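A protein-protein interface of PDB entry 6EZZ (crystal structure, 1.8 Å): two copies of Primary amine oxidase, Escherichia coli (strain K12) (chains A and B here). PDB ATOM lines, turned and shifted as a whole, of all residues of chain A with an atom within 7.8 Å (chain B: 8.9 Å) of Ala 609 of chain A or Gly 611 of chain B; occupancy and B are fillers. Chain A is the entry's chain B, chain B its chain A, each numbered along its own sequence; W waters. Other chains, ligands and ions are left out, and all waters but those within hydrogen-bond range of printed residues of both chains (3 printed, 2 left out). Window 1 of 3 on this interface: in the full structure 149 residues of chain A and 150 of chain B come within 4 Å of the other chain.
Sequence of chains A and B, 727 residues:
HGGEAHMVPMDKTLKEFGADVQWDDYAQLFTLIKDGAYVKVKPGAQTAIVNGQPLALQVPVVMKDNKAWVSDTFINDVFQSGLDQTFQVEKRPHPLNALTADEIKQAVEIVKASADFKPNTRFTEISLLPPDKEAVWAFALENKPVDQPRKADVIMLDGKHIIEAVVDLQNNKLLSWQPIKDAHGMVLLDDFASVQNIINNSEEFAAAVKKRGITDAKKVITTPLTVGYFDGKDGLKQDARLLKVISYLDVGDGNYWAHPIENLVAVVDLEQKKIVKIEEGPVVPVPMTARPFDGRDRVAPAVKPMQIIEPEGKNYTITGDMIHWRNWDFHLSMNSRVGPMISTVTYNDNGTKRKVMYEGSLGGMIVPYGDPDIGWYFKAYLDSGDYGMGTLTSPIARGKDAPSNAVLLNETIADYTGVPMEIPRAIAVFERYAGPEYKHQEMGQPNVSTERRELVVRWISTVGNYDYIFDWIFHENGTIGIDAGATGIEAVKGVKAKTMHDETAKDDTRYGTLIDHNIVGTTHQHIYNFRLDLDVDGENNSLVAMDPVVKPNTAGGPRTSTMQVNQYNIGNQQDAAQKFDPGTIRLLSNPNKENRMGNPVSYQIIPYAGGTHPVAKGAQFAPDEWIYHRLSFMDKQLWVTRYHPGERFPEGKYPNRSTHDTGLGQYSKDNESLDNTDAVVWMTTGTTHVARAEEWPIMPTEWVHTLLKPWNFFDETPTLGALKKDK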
ATOM      1  N   ILE A 482      24.620  18.086   0.758  1.00  0.00           N
ATOM      2  CA  ILE A 482      23.953  18.211  -0.527  1.00  0.00           C
ATOM      3  C   ILE A 482      22.741  17.287  -0.481  1.00  0.00           C
ATOM      4  O   ILE A 482      22.894  16.048  -0.348  1.00  0.00           O
ATOM      5  CB  ILE A 482      24.830  17.868  -1.744  1.00  0.00           C
ATOM      6  CG1 ILE A 482      26.175  18.588  -1.682  1.00  0.00           C
ATOM      7  CG2 ILE A 482      24.096  18.217  -3.035  1.00  0.00           C
ATOM      8  CD1 ILE A 482      27.236  18.028  -2.608  1.00  0.00           C
ATOM      9  N   ASP A 483      21.561  17.891  -0.547  1.00  0.00           N
ATOM     10  CA  ASP A 483      20.298  17.143  -0.456  1.00  0.00           C
ATOM     11  C   ASP A 483      19.526  17.316  -1.729  1.00  0.00           C
ATOM     12  O   ASP A 483      19.546  18.415  -2.315  1.00  0.00           O
ATOM     13  CB  ASP A 483      19.457  17.619   0.709  1.00  0.00           C
ATOM     14  CG  ASP A 483      20.036  17.238   2.083  1.00  0.00           C
ATOM     15  OD1 ASP A 483      21.133  16.648   2.215  1.00  0.00           O
ATOM     16  OD2 ASP A 483      19.369  17.596   3.062  1.00  0.00           O
ATOM     17  N   PHE A 580      29.400   2.221  -2.042  1.00  0.00           N
ATOM     18  CA  PHE A 580      29.642   2.855  -0.746  1.00  0.00           C
ATOM     19  C   PHE A 580      28.945   2.081   0.345  1.00  0.00           C
ATOM     20  O   PHE A 580      27.707   1.937   0.329  1.00  0.00           O
ATOM     21  CB  PHE A 580      29.143   4.291  -0.742  1.00  0.00           C
ATOM     22  CG  PHE A 580      29.330   4.982   0.577  1.00  0.00           C
ATOM     23  CD1 PHE A 580      30.606   5.245   1.056  1.00  0.00           C
ATOM     24  CD2 PHE A 580      28.224   5.362   1.351  1.00  0.00           C
ATOM     25  CE1 PHE A 580      30.792   5.876   2.284  1.00  0.00           C
ATOM     26  CE2 PHE A 580      28.408   5.989   2.585  1.00  0.00           C
ATOM     27  CZ  PHE A 580      29.687   6.255   3.047  1.00  0.00           C
ATOM     28  N   PRO A 582      28.038   2.459   4.072  1.00  0.00           N
ATOM     29  CA  PRO A 582      27.924   3.579   5.015  1.00  0.00           C
ATOM     30  C   PRO A 582      28.504   3.296   6.402  1.00  0.00           C
ATOM     31  O   PRO A 582      28.570   4.218   7.232  1.00  0.00           O
ATOM     32  CB  PRO A 582      26.398   3.835   5.072  1.00  0.00           C
ATOM     33  CG  PRO A 582      25.789   2.510   4.768  1.00  0.00           C
ATOM     34  CD  PRO A 582      26.714   1.848   3.790  1.00  0.00           C
ATOM     35  N   ILE A 606      30.531  11.245   2.116  1.00  0.00           N
ATOM     36  CA  ILE A 606      29.393  10.390   2.501  1.00  0.00           C
ATOM     37  C   ILE A 606      28.326  10.503   1.406  1.00  0.00           C
ATOM     38  O   ILE A 606      27.493  11.426   1.437  1.00  0.00           O
ATOM     39  CB  ILE A 606      28.790  10.756   3.877  1.00  0.00           C
ATOM     40  CG1 ILE A 606      29.904  10.820   4.932  1.00  0.00           C
ATOM     41  CG2 ILE A 606      27.678   9.761   4.263  1.00  0.00           C
ATOM     42  CD1 ILE A 606      29.499  11.142   6.323  1.00  0.00           C
ATOM     43  N   PRO A 607      28.366   9.593   0.407  1.00  0.00           N
ATOM     44  CA  PRO A 607      27.395   9.639  -0.705  1.00  0.00           C
ATOM     45  C   PRO A 607      26.009   9.202  -0.281  1.00  0.00           C
ATOM     46  O   PRO A 607      25.070   9.454  -0.999  1.00  0.00           O
ATOM     47  CB  PRO A 607      27.945   8.626  -1.735  1.00  0.00           C
ATOM     48  CG  PRO A 607      29.324   8.299  -1.289  1.00  0.00           C
ATOM     49  CD  PRO A 607      29.470   8.638   0.147  1.00  0.00           C
ATOM     50  N   TYR A 608      25.910   8.469   0.814  1.00  0.00           N
ATOM     51  CA  TYR A 608      24.612   8.072   1.358  1.00  0.00           C
ATOM     52  C   TYR A 608      24.548   8.407   2.827  1.00  0.00           C
ATOM     53  O   TYR A 608      25.102   7.673   3.670  1.00  0.00           O
ATOM     54  CB  TYR A 608      24.287   6.573   1.155  1.00  0.00           C
ATOM     55  CG  TYR A 608      22.832   6.319   1.568  1.00  0.00           C
ATOM     56  CD1 TYR A 608      21.797   6.955   0.887  1.00  0.00           C
ATOM     57  CD2 TYR A 608      22.490   5.498   2.657  1.00  0.00           C
ATOM     58  CE1 TYR A 608      20.465   6.787   1.246  1.00  0.00           C
ATOM     59  CE2 TYR A 608      21.143   5.313   3.013  1.00  0.00           C
ATOM     60  CZ  TYR A 608      20.141   5.975   2.305  1.00  0.00           C
ATOM     61  OH  TYR A 608      18.787   5.849   2.610  1.00  0.00           O
ATOM     62  N   ALA A 609      23.876   9.528   3.136  1.00  0.00           N
ATOM     63  CA  ALA A 609      23.615   9.945   4.507  1.00  0.00           C
ATOM     64  C   ALA A 609      22.133   9.859   4.831  1.00  0.00           C
ATOM     65  O   ALA A 609      21.679  10.430   5.837  1.00  0.00           O
ATOM     66  CB  ALA A 609      24.108  11.359   4.763  1.00  0.00           C
ATOM     67  N   GLY A 610      21.394   9.139   4.002  1.00  0.00           N
ATOM     68  CA  GLY A 610      19.982   8.879   4.303  1.00  0.00           C
ATOM     69  C   GLY A 610      19.034   9.274   3.234  1.00  0.00           C
ATOM     70  O   GLY A 610      19.413   9.831   2.227  1.00  0.00           O
ATOM     71  N   GLY A 611      17.780   8.926   3.460  1.00  0.00           N
ATOM     72  CA  GLY A 611      16.723   9.273   2.550  1.00  0.00           C
ATOM     73  C   GLY A 611      15.398   8.702   3.013  1.00  0.00           C
ATOM     74  O   GLY A 611      15.351   7.859   3.899  1.00  0.00           O
ATOM     75  N   THR A 685      23.843   8.883  -5.781  1.00  0.00           N
ATOM     76  CA  THR A 685      22.881   8.493  -4.770  1.00  0.00           C
ATOM     77  C   THR A 685      21.541   8.326  -5.438  1.00  0.00           C
ATOM     78  O   THR A 685      21.116   9.137  -6.274  1.00  0.00           O
ATOM     79  CB  THR A 685      22.821   9.495  -3.582  1.00  0.00           C
ATOM     80  OG1 THR A 685      21.883   9.034  -2.607  1.00  0.00           O
ATOM     81  CG2 THR A 685      22.438  10.875  -4.004  1.00  0.00           C
ATOM     82  N   VAL A 704      16.762  12.762  -0.323  1.00  0.00           N
ATOM     83  CA  VAL A 704      17.996  12.021  -0.040  1.00  0.00           C
ATOM     84  C   VAL A 704      19.067  13.005   0.388  1.00  0.00           C
ATOM     85  O   VAL A 704      19.036  14.167  -0.040  1.00  0.00           O
ATOM     86  CB  VAL A 704      18.519  11.160  -1.225  1.00  0.00           C
ATOM     87  CG1 VAL A 704      17.484  10.102  -1.592  1.00  0.00           C
ATOM     88  CG2 VAL A 704      18.826  12.001  -2.449  1.00  0.00           C
ATOM     89  N   HIS A 705      20.005  12.528   1.201  1.00  0.00           N
ATOM     90  CA  HIS A 705      20.995  13.395   1.859  1.00  0.00           C
ATOM     91  C   HIS A 705      22.384  12.850   1.613  1.00  0.00           C
ATOM     92  O   HIS A 705      22.578  11.626   1.612  1.00  0.00           O
ATOM     93  CB  HIS A 705      20.760  13.481   3.382  1.00  0.00           C
ATOM     94  CG  HIS A 705      19.331  13.640   3.774  1.00  0.00           C
ATOM     95  ND1 HIS A 705      18.658  14.840   3.681  1.00  0.00           N
ATOM     96  CD2 HIS A 705      18.448  12.747   4.293  1.00  0.00           C
ATOM     97  CE1 HIS A 705      17.417  14.671   4.096  1.00  0.00           C
ATOM     98  NE2 HIS A 705      17.257  13.410   4.454  1.00  0.00           N
ATOM     99  N   THR A 706      23.337  13.758   1.413  1.00  0.00           N
ATOM    100  CA  THR A 706      24.747  13.425   1.274  1.00  0.00           C
ATOM    101  C   THR A 706      25.525  14.450   2.100  1.00  0.00           C
ATOM    102  O   THR A 706      25.010  15.540   2.401  1.00  0.00           O
ATOM    103  CB  THR A 706      25.239  13.449  -0.198  1.00  0.00           C
ATOM    104  OG1 THR A 706      25.386  14.796  -0.652  1.00  0.00           O
ATOM    105  CG2 THR A 706      24.286  12.703  -1.172  1.00  0.00           C
ATOM    106  N   LEU A 707      26.752  14.102   2.483  1.00  0.00           N
ATOM    107  CA  LEU A 707      27.570  14.944   3.337  1.00  0.00           C
ATOM    108  C   LEU A 707      29.045  14.910   3.011  1.00  0.00           C
ATOM    109  O   LEU A 707      29.576  13.879   2.667  1.00  0.00           O
ATOM    110  CB  LEU A 707      27.467  14.514   4.785  1.00  0.00           C
ATOM    111  CG  LEU A 707      26.289  14.874   5.635  1.00  0.00           C
ATOM    112  CD1 LEU A 707      26.496  14.269   7.016  1.00  0.00           C
ATOM    113  CD2 LEU A 707      26.018  16.372   5.771  1.00  0.00           C
ATOM    114  N   LEU A 708      29.682  16.055   3.209  1.00  0.00           N
ATOM    115  CA  LEU A 708      31.125  16.194   3.200  1.00  0.00           C
ATOM    116  C   LEU A 708      31.543  16.812   4.531  1.00  0.00           C
ATOM    117  O   LEU A 708      31.085  17.919   4.882  1.00  0.00           O
ATOM    118  CB  LEU A 708      31.534  17.098   2.052  1.00  0.00           C
ATOM    119  CG  LEU A 708      30.953  16.769   0.690  1.00  0.00           C
ATOM    120  CD1 LEU A 708      31.204  17.958  -0.217  1.00  0.00           C
ATOM    121  CD2 LEU A 708      31.630  15.510   0.134  1.00  0.00           C
ATOM    122  N   LYS A 709      32.367  16.119   5.312  1.00  0.00           N
ATOM    123  CA  LYS A 709      32.630  16.569   6.672  1.00  0.00           C
ATOM    124  C   LYS A 709      34.126  16.773   6.834  1.00  0.00           C
ATOM    125  O   LYS A 709      34.864  15.876   6.445  1.00  0.00           O
ATOM    126  CB  LYS A 709      32.196  15.559   7.732  1.00  0.00           C
ATOM    127  CG  LYS A 709      30.713  15.203   7.745  1.00  0.00           C
ATOM    128  CD  LYS A 709      30.428  14.059   8.709  1.00  0.00           C
ATOM    129  CE  LYS A 709      30.468  14.521  10.144  1.00  0.00           C
ATOM    130  NZ  LYS A 709      30.137  13.454  11.112  1.00  0.00           N
ATOM    131  N   ASP B 483      14.172  10.899  15.490  1.00  0.00           N
ATOM    132  CA  ASP B 483      15.574  11.240  15.289  1.00  0.00           C
ATOM    133  C   ASP B 483      16.249  11.288  16.635  1.00  0.00           C
ATOM    134  O   ASP B 483      15.648  11.684  17.632  1.00  0.00           O
ATOM    135  CB  ASP B 483      15.703  12.601  14.595  1.00  0.00           C
ATOM    136  CG  ASP B 483      15.344  12.556  13.084  1.00  0.00           C
ATOM    137  OD1 ASP B 483      14.868  11.560  12.555  1.00  0.00           O
ATOM    138  OD2 ASP B 483      15.561  13.566  12.397  1.00  0.00           O
ATOM    139  N   ALA B 484      17.507  10.860  16.659  1.00  0.00           N
ATOM    140  CA  ALA B 484      18.297  10.839  17.862  1.00  0.00           C
ATOM    141  C   ALA B 484      19.603  11.544  17.605  1.00  0.00           C
ATOM    142  O   ALA B 484      20.308  11.208  16.658  1.00  0.00           O
ATOM    143  CB  ALA B 484      18.542   9.420  18.319  1.00  0.00           C
ATOM    144  N   PRO B 607      13.950   1.599   9.966  1.00  0.00           N
ATOM    145  CA  PRO B 607      14.847   1.771  11.128  1.00  0.00           C
ATOM    146  C   PRO B 607      16.125   2.544  10.815  1.00  0.00           C
ATOM    147  O   PRO B 607      16.830   2.976  11.723  1.00  0.00           O
ATOM    148  CB  PRO B 607      15.209   0.338  11.532  1.00  0.00           C
ATOM    149  CG  PRO B 607      14.329  -0.567  10.759  1.00  0.00           C
ATOM    150  CD  PRO B 607      13.744   0.183   9.602  1.00  0.00           C
ATOM    151  N   TYR B 608      16.465   2.648   9.543  1.00  0.00           N
ATOM    152  CA  TYR B 608      17.644   3.413   9.137  1.00  0.00           C
ATOM    153  C   TYR B 608      17.246   4.297   7.994  1.00  0.00           C
ATOM    154  O   TYR B 608      17.145   3.822   6.866  1.00  0.00           O
ATOM    155  CB  TYR B 608      18.787   2.494   8.749  1.00  0.00           C
ATOM    156  CG  TYR B 608      19.932   3.224   8.104  1.00  0.00           C
ATOM    157  CD1 TYR B 608      20.658   4.203   8.785  1.00  0.00           C
ATOM    158  CD2 TYR B 608      20.279   2.932   6.788  1.00  0.00           C
ATOM    159  CE1 TYR B 608      21.697   4.878   8.160  1.00  0.00           C
ATOM    160  CE2 TYR B 608      21.314   3.581   6.164  1.00  0.00           C
ATOM    161  CZ  TYR B 608      22.013   4.542   6.840  1.00  0.00           C
ATOM    162  OH  TYR B 608      23.029   5.127   6.122  1.00  0.00           O
ATOM    163  N   ALA B 609      16.979   5.573   8.298  1.00  0.00           N
ATOM    164  CA  ALA B 609      16.706   6.607   7.286  1.00  0.00           C
ATOM    165  C   ALA B 609      17.882   7.596   7.203  1.00  0.00           C
ATOM    166  O   ALA B 609      17.762   8.655   6.591  1.00  0.00           O
ATOM    167  CB  ALA B 609      15.421   7.342   7.610  1.00  0.00           C
ATOM    168  N   GLY B 610      19.021   7.225   7.774  1.00  0.00           N
ATOM    169  CA  GLY B 610      20.255   7.982   7.584  1.00  0.00           C
ATOM    170  C   GLY B 610      20.905   8.399   8.875  1.00  0.00           C
ATOM    171  O   GLY B 610      20.441   8.072   9.978  1.00  0.00           O
ATOM    172  N   GLY B 611      22.006   9.103   8.710  1.00  0.00           N
ATOM    173  CA  GLY B 611      22.788   9.581   9.820  1.00  0.00           C
ATOM    174  C   GLY B 611      24.051  10.280   9.362  1.00  0.00           C
ATOM    175  O   GLY B 611      24.456  10.155   8.205  1.00  0.00           O
ATOM    176  N   THR B 612      24.665  11.007  10.289  1.00  0.00           N
ATOM    177  CA  THR B 612      25.810  11.839  10.026  1.00  0.00           C
ATOM    178  C   THR B 612      27.129  11.228  10.484  1.00  0.00           C
ATOM    179  O   THR B 612      28.169  11.738  10.127  1.00  0.00           O
ATOM    180  CB  THR B 612      25.568  13.235  10.673  1.00  0.00           C
ATOM    181  OG1 THR B 612      25.393  13.088  12.087  1.00  0.00           O
ATOM    182  CG2 THR B 612      24.266  13.876  10.099  1.00  0.00           C
ATOM    183  N   HIS B 613      27.083  10.148  11.281  1.00  0.00           N
ATOM    184  CA  HIS B 613      28.246   9.330  11.609  1.00  0.00           C
ATOM    185  C   HIS B 613      28.146   8.010  10.834  1.00  0.00           C
ATOM    186  O   HIS B 613      27.077   7.625  10.346  1.00  0.00           O
ATOM    187  CB  HIS B 613      28.270   8.966  13.104  1.00  0.00           C
ATOM    188  CG  HIS B 613      29.039   9.901  13.999  1.00  0.00           C
ATOM    189  ND1 HIS B 613      30.072  10.712  13.574  1.00  0.00           N
ATOM    190  CD2 HIS B 613      28.986  10.045  15.340  1.00  0.00           C
ATOM    191  CE1 HIS B 613      30.582  11.358  14.613  1.00  0.00           C
ATOM    192  NE2 HIS B 613      29.929  10.978  15.695  1.00  0.00           N
ATOM    193  N   PRO B 614      29.257   7.278  10.733  1.00  0.00           N
ATOM    194  CA  PRO B 614      29.139   5.970  10.074  1.00  0.00           C
ATOM    195  C   PRO B 614      28.113   5.047  10.751  1.00  0.00           C
ATOM    196  O   PRO B 614      27.979   5.047  11.995  1.00  0.00           O
ATOM    197  CB  PRO B 614      30.545   5.399  10.219  1.00  0.00           C
ATOM    198  CG  PRO B 614      31.424   6.590  10.321  1.00  0.00           C
ATOM    199  CD  PRO B 614      30.631   7.555  11.149  1.00  0.00           C
ATOM    200  N   VAL B 615      27.435   4.225   9.955  1.00  0.00           N
ATOM    201  CA  VAL B 615      26.319   3.392  10.438  1.00  0.00           C
ATOM    202  C   VAL B 615      26.856   2.067  10.963  1.00  0.00           C
ATOM    203  O   VAL B 615      27.798   1.509  10.431  1.00  0.00           O
ATOM    204  CB  VAL B 615      25.322   3.052   9.331  1.00  0.00           C
ATOM    205  CG1 VAL B 615      24.029   2.482   9.914  1.00  0.00           C
ATOM    206  CG2 VAL B 615      25.006   4.282   8.505  1.00  0.00           C
ATOM    207  N   THR B 685      18.821   1.365  15.949  1.00  0.00           N
ATOM    208  CA  THR B 685      19.642   2.127  15.018  1.00  0.00           C
ATOM    209  C   THR B 685      20.903   2.558  15.704  1.00  0.00           C
ATOM    210  O   THR B 685      20.891   2.945  16.855  1.00  0.00           O
ATOM    211  CB  THR B 685      18.878   3.343  14.419  1.00  0.00           C
ATOM    212  OG1 THR B 685      19.671   3.948  13.406  1.00  0.00           O
ATOM    213  CG2 THR B 685      18.573   4.380  15.423  1.00  0.00           C
ATOM    214  N   GLY B 686      22.015   2.490  15.016  1.00  0.00           N
ATOM    215  CA  GLY B 686      23.246   2.870  15.667  1.00  0.00           C
ATOM    216  C   GLY B 686      24.335   3.349  14.751  1.00  0.00           C
ATOM    217  O   GLY B 686      24.262   3.175  13.524  1.00  0.00           O
ATOM    218  N   THR B 687      25.347   3.933  15.374  1.00  0.00           N
ATOM    219  CA  THR B 687      26.506   4.427  14.674  1.00  0.00           C
ATOM    220  C   THR B 687      27.774   3.789  15.229  1.00  0.00           C
ATOM    221  O   THR B 687      27.789   3.325  16.348  1.00  0.00           O
ATOM    222  CB  THR B 687      26.630   5.946  14.848  1.00  0.00           C
ATOM    223  OG1 THR B 687      26.780   6.256  16.239  1.00  0.00           O
ATOM    224  CG2 THR B 687      25.392   6.642  14.292  1.00  0.00           C
ATOM    225  N   GLU B 702      25.596  15.242  16.323  1.00  0.00           N
ATOM    226  CA  GLU B 702      25.449  14.290  15.216  1.00  0.00           C
ATOM    227  C   GLU B 702      24.076  13.613  15.316  1.00  0.00           C
ATOM    228  O   GLU B 702      23.657  13.298  16.403  1.00  0.00           O
ATOM    229  CB  GLU B 702      26.525  13.219  15.327  1.00  0.00           C
ATOM    230  CG  GLU B 702      27.952  13.790  15.317  1.00  0.00           C
ATOM    231  CD  GLU B 702      28.511  14.017  13.925  1.00  0.00           C
ATOM    232  OE1 GLU B 702      27.757  13.849  12.924  1.00  0.00           O
ATOM    233  OE2 GLU B 702      29.729  14.401  13.832  1.00  0.00           O
ATOM    234  N   TRP B 703      23.443  13.316  14.192  1.00  0.00           N
ATOM    235  CA  TRP B 703      22.054  12.802  14.188  1.00  0.00           C
ATOM    236  C   TRP B 703      21.938  11.490  13.439  1.00  0.00           C
ATOM    237  O   TRP B 703      22.697  11.247  12.502  1.00  0.00           O
ATOM    238  CB  TRP B 703      21.151  13.815  13.494  1.00  0.00           C
ATOM    239  CG  TRP B 703      20.924  15.100  14.278  1.00  0.00           C
ATOM    240  CD1 TRP B 703      21.620  16.264  14.166  1.00  0.00           C
ATOM    241  CD2 TRP B 703      19.920  15.319  15.261  1.00  0.00           C
ATOM    242  NE1 TRP B 703      21.106  17.211  15.007  1.00  0.00           N
ATOM    243  CE2 TRP B 703      20.060  16.656  15.705  1.00  0.00           C
ATOM    244  CE3 TRP B 703      18.884  14.525  15.791  1.00  0.00           C
ATOM    245  CZ2 TRP B 703      19.224  17.215  16.646  1.00  0.00           C
ATOM    246  CZ3 TRP B 703      18.073  15.059  16.757  1.00  0.00           C
ATOM    247  CH2 TRP B 703      18.235  16.402  17.188  1.00  0.00           C
ATOM    248  N   VAL B 704      20.962  10.681  13.855  1.00  0.00           N
ATOM    249  CA  VAL B 704      20.459   9.523  13.114  1.00  0.00           C
ATOM    250  C   VAL B 704      18.946   9.684  12.969  1.00  0.00           C
ATOM    251  O   VAL B 704      18.313  10.306  13.813  1.00  0.00           O
ATOM    252  CB  VAL B 704      20.781   8.167  13.782  1.00  0.00           C
ATOM    253  CG1 VAL B 704      22.277   8.007  13.939  1.00  0.00           C
ATOM    254  CG2 VAL B 704      20.124   8.032  15.136  1.00  0.00           C
ATOM    255  N   HIS B 705      18.398   9.126  11.894  1.00  0.00           N
ATOM    256  CA  HIS B 705      17.025   9.355  11.489  1.00  0.00           C
ATOM    257  C   HIS B 705      16.325   8.027  11.291  1.00  0.00           C
ATOM    258  O   HIS B 705      16.899   7.094  10.763  1.00  0.00           O
ATOM    259  CB  HIS B 705      16.962  10.138  10.170  1.00  0.00           C
ATOM    260  CG  HIS B 705      17.854  11.328  10.134  1.00  0.00           C
ATOM    261  ND1 HIS B 705      17.572  12.484  10.824  1.00  0.00           N
ATOM    262  CD2 HIS B 705      19.051  11.521   9.540  1.00  0.00           C
ATOM    263  CE1 HIS B 705      18.529  13.363  10.596  1.00  0.00           C
ATOM    264  NE2 HIS B 705      19.449  12.797   9.843  1.00  0.00           N
ATOM    265  N   THR B 706      15.075   7.945  11.732  1.00  0.00           N
ATOM    266  CA  THR B 706      14.207   6.809  11.430  1.00  0.00           C
ATOM    267  C   THR B 706      12.850   7.331  11.008  1.00  0.00           C
ATOM    268  O   THR B 706      12.520   8.482  11.286  1.00  0.00           O
ATOM    269  CB  THR B 706      13.996   5.893  12.651  1.00  0.00           C
ATOM    270  OG1 THR B 706      13.134   6.525  13.580  1.00  0.00           O
ATOM    271  CG2 THR B 706      15.340   5.524  13.329  1.00  0.00           C
HETATM  272  O   HOH W   1      21.587  12.728   7.317  1.00  0.00           O
HETATM  273  O   HOH W   2      15.930  10.832   6.210  1.00  0.00           O
HETATM  274  O   HOH W   3      32.275  11.451  11.056  1.00  0.00           O
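The backbone NH (N) of Ala 609 of chain B is in hydrogen-bond range of the backbone carbonyl oxygen (O) of His 705 of chain B (2.9 Å).
The backbone carbonyl oxygen of Gly 610 of chain B is in hydrogen-bond range of the backbone NH of His 705 of chain B (3.0 Å).
The side-chain hydroxyl (OG1) of Thr 612 of chain B is in hydrogen-bond range of the side-chain carboxylate (OE1) of Glu 702 of chain B.
The side-chain hydroxyl (OG1) of Thr 612 of chain B sits at hydrogen-bond distance from the backbone NH (N) of Trp 703 of chain B (2.9 Å).
The side-chain hydroxyl (OH) of Tyr 608 of chain A is in hydrogen-bond range of the backbone NH (N) of Gly 611 of chain A (3.3 Å).
N of His 705 of chain A sits at hydrogen-bond distance from O of Gly 610 of chain A, 2.9 Å away.
Among the printed residues, pairs that only touch across the chains: Pro 582 of chain A with Tyr 608 of chain B, Pro 582 of chain A with Pro 614 of chain B, Tyr 608 of chain A with Tyr 608 of chain B, Ala 609 of chain A with Gly 610 of chain B, Gly 610 of chain A with Ala 609 of chain B, Gly 610 of chain A with Gly 610 of chain B, Leu 707 of chain A with Thr 612 of chain B and Lys 709 of chain A with His 613 of chain B.
Of chain B, only Gly 610 (3.3 Å) and Gly 611 (3.2 Å) come within 4 Å of Ala 609 of chain A.
Gly 611 of chain B touches just one residue of chain A: Ala 609.
Gly 610 of chain B touches just these residues of chain A: Ala 609 (3.3 Å) and Gly 610 (3.4 Å).
Printed residues of chain A within 4 Å of His 613 of chain B: Lys 709 (3.7 Å).
Printed residues of chain B within 4 Å of Pro 582 of chain A: Tyr 608, Pro 614 and Val 615.
Printed residues of chain A within 4 Å of Tyr 608 of chain B: Pro 582 (3.8 Å) and Tyr 608 (3.5 Å).
Of the printed residues of chain A, Thr 612 of chain B touches Leu 707 and Lys 709.
The nearest residue of chain B that does not touch Ala 609 of chain A is Ala 609 of chain B (4.4 Å).
The nearest printed residue of chain B that does not touch Leu 707 of chain A is Gly 611 of chain B (4.7 Å).
N of Gly 611 of chain A is in hydrogen-bond range of O of Ala 609 of chain B (3.1 Å).
O of Ala 609 of chain A sits at hydrogen-bond distance from N of Gly 611 of chain B, 3.2 Å away.
NZ of Lys 709 of chain A lies within hydrogen-bond range of O of Thr 612 of chain B, 2.8 Å away.
The backbone NH of Val 615 of chain B sits at hydrogen-bond distance from the backbone carbonyl oxygen of Pro 582 of chain A.
OE2 of Glu 702 of chain B lies within salt-bridge range of NZ of Lys 709 of chain A, 2.9 Å away.
Tyr 608 of chain B touches its own counterpart, Tyr 608 of chain A.
Ala 609 of chain A touches Gly 610 of chain B, and with the chains exchanged Gly 610 of chain A touches Ala 609 of chain B.
Ala 609 of chain A touches Gly 611 of chain B, and with the chains exchanged Gly 611 of chain A touches Ala 609 of chain B.
Gly 610 of chain A touches its own counterpart, Gly 610 of chain B.
10 positions are printed for both chains.
Water W1 lies within hydrogen-bond range of O of Ala 609 of chain A (2.7 Å) and NE2 of His 705 of chain B (3.3 Å).
Water W2 bridges the backbone carbonyl oxygen of Ala 609 of chain B (2.9 Å) and a ring nitrogen (NE2) of His 705 of chain A (3.4 Å).
Water W3 lies within hydrogen-bond range of NZ of Lys 709 of chain A and ND1 of His 613 of chain B.
Printed residues of chain A that touch a printed residue of chain B: Pro 582, Tyr 608, Ala 609, Gly 610, Gly 611, Leu 707 and Lys 709.
Hydrophobic or aromatic side chains of chain A that line the printed part of chain B: Pro 582, Tyr 608, Ala 609 and Leu 707.
Along chain A the printed residues that touch a printed residue of chain B span positions 582 to 709.
Among the printed residues, Asp or Glu carboxylates within 4 Å of a Lys or Arg side-chain nitrogen of the other chain: Lys 709 of chain A with Glu 702 of chain B.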
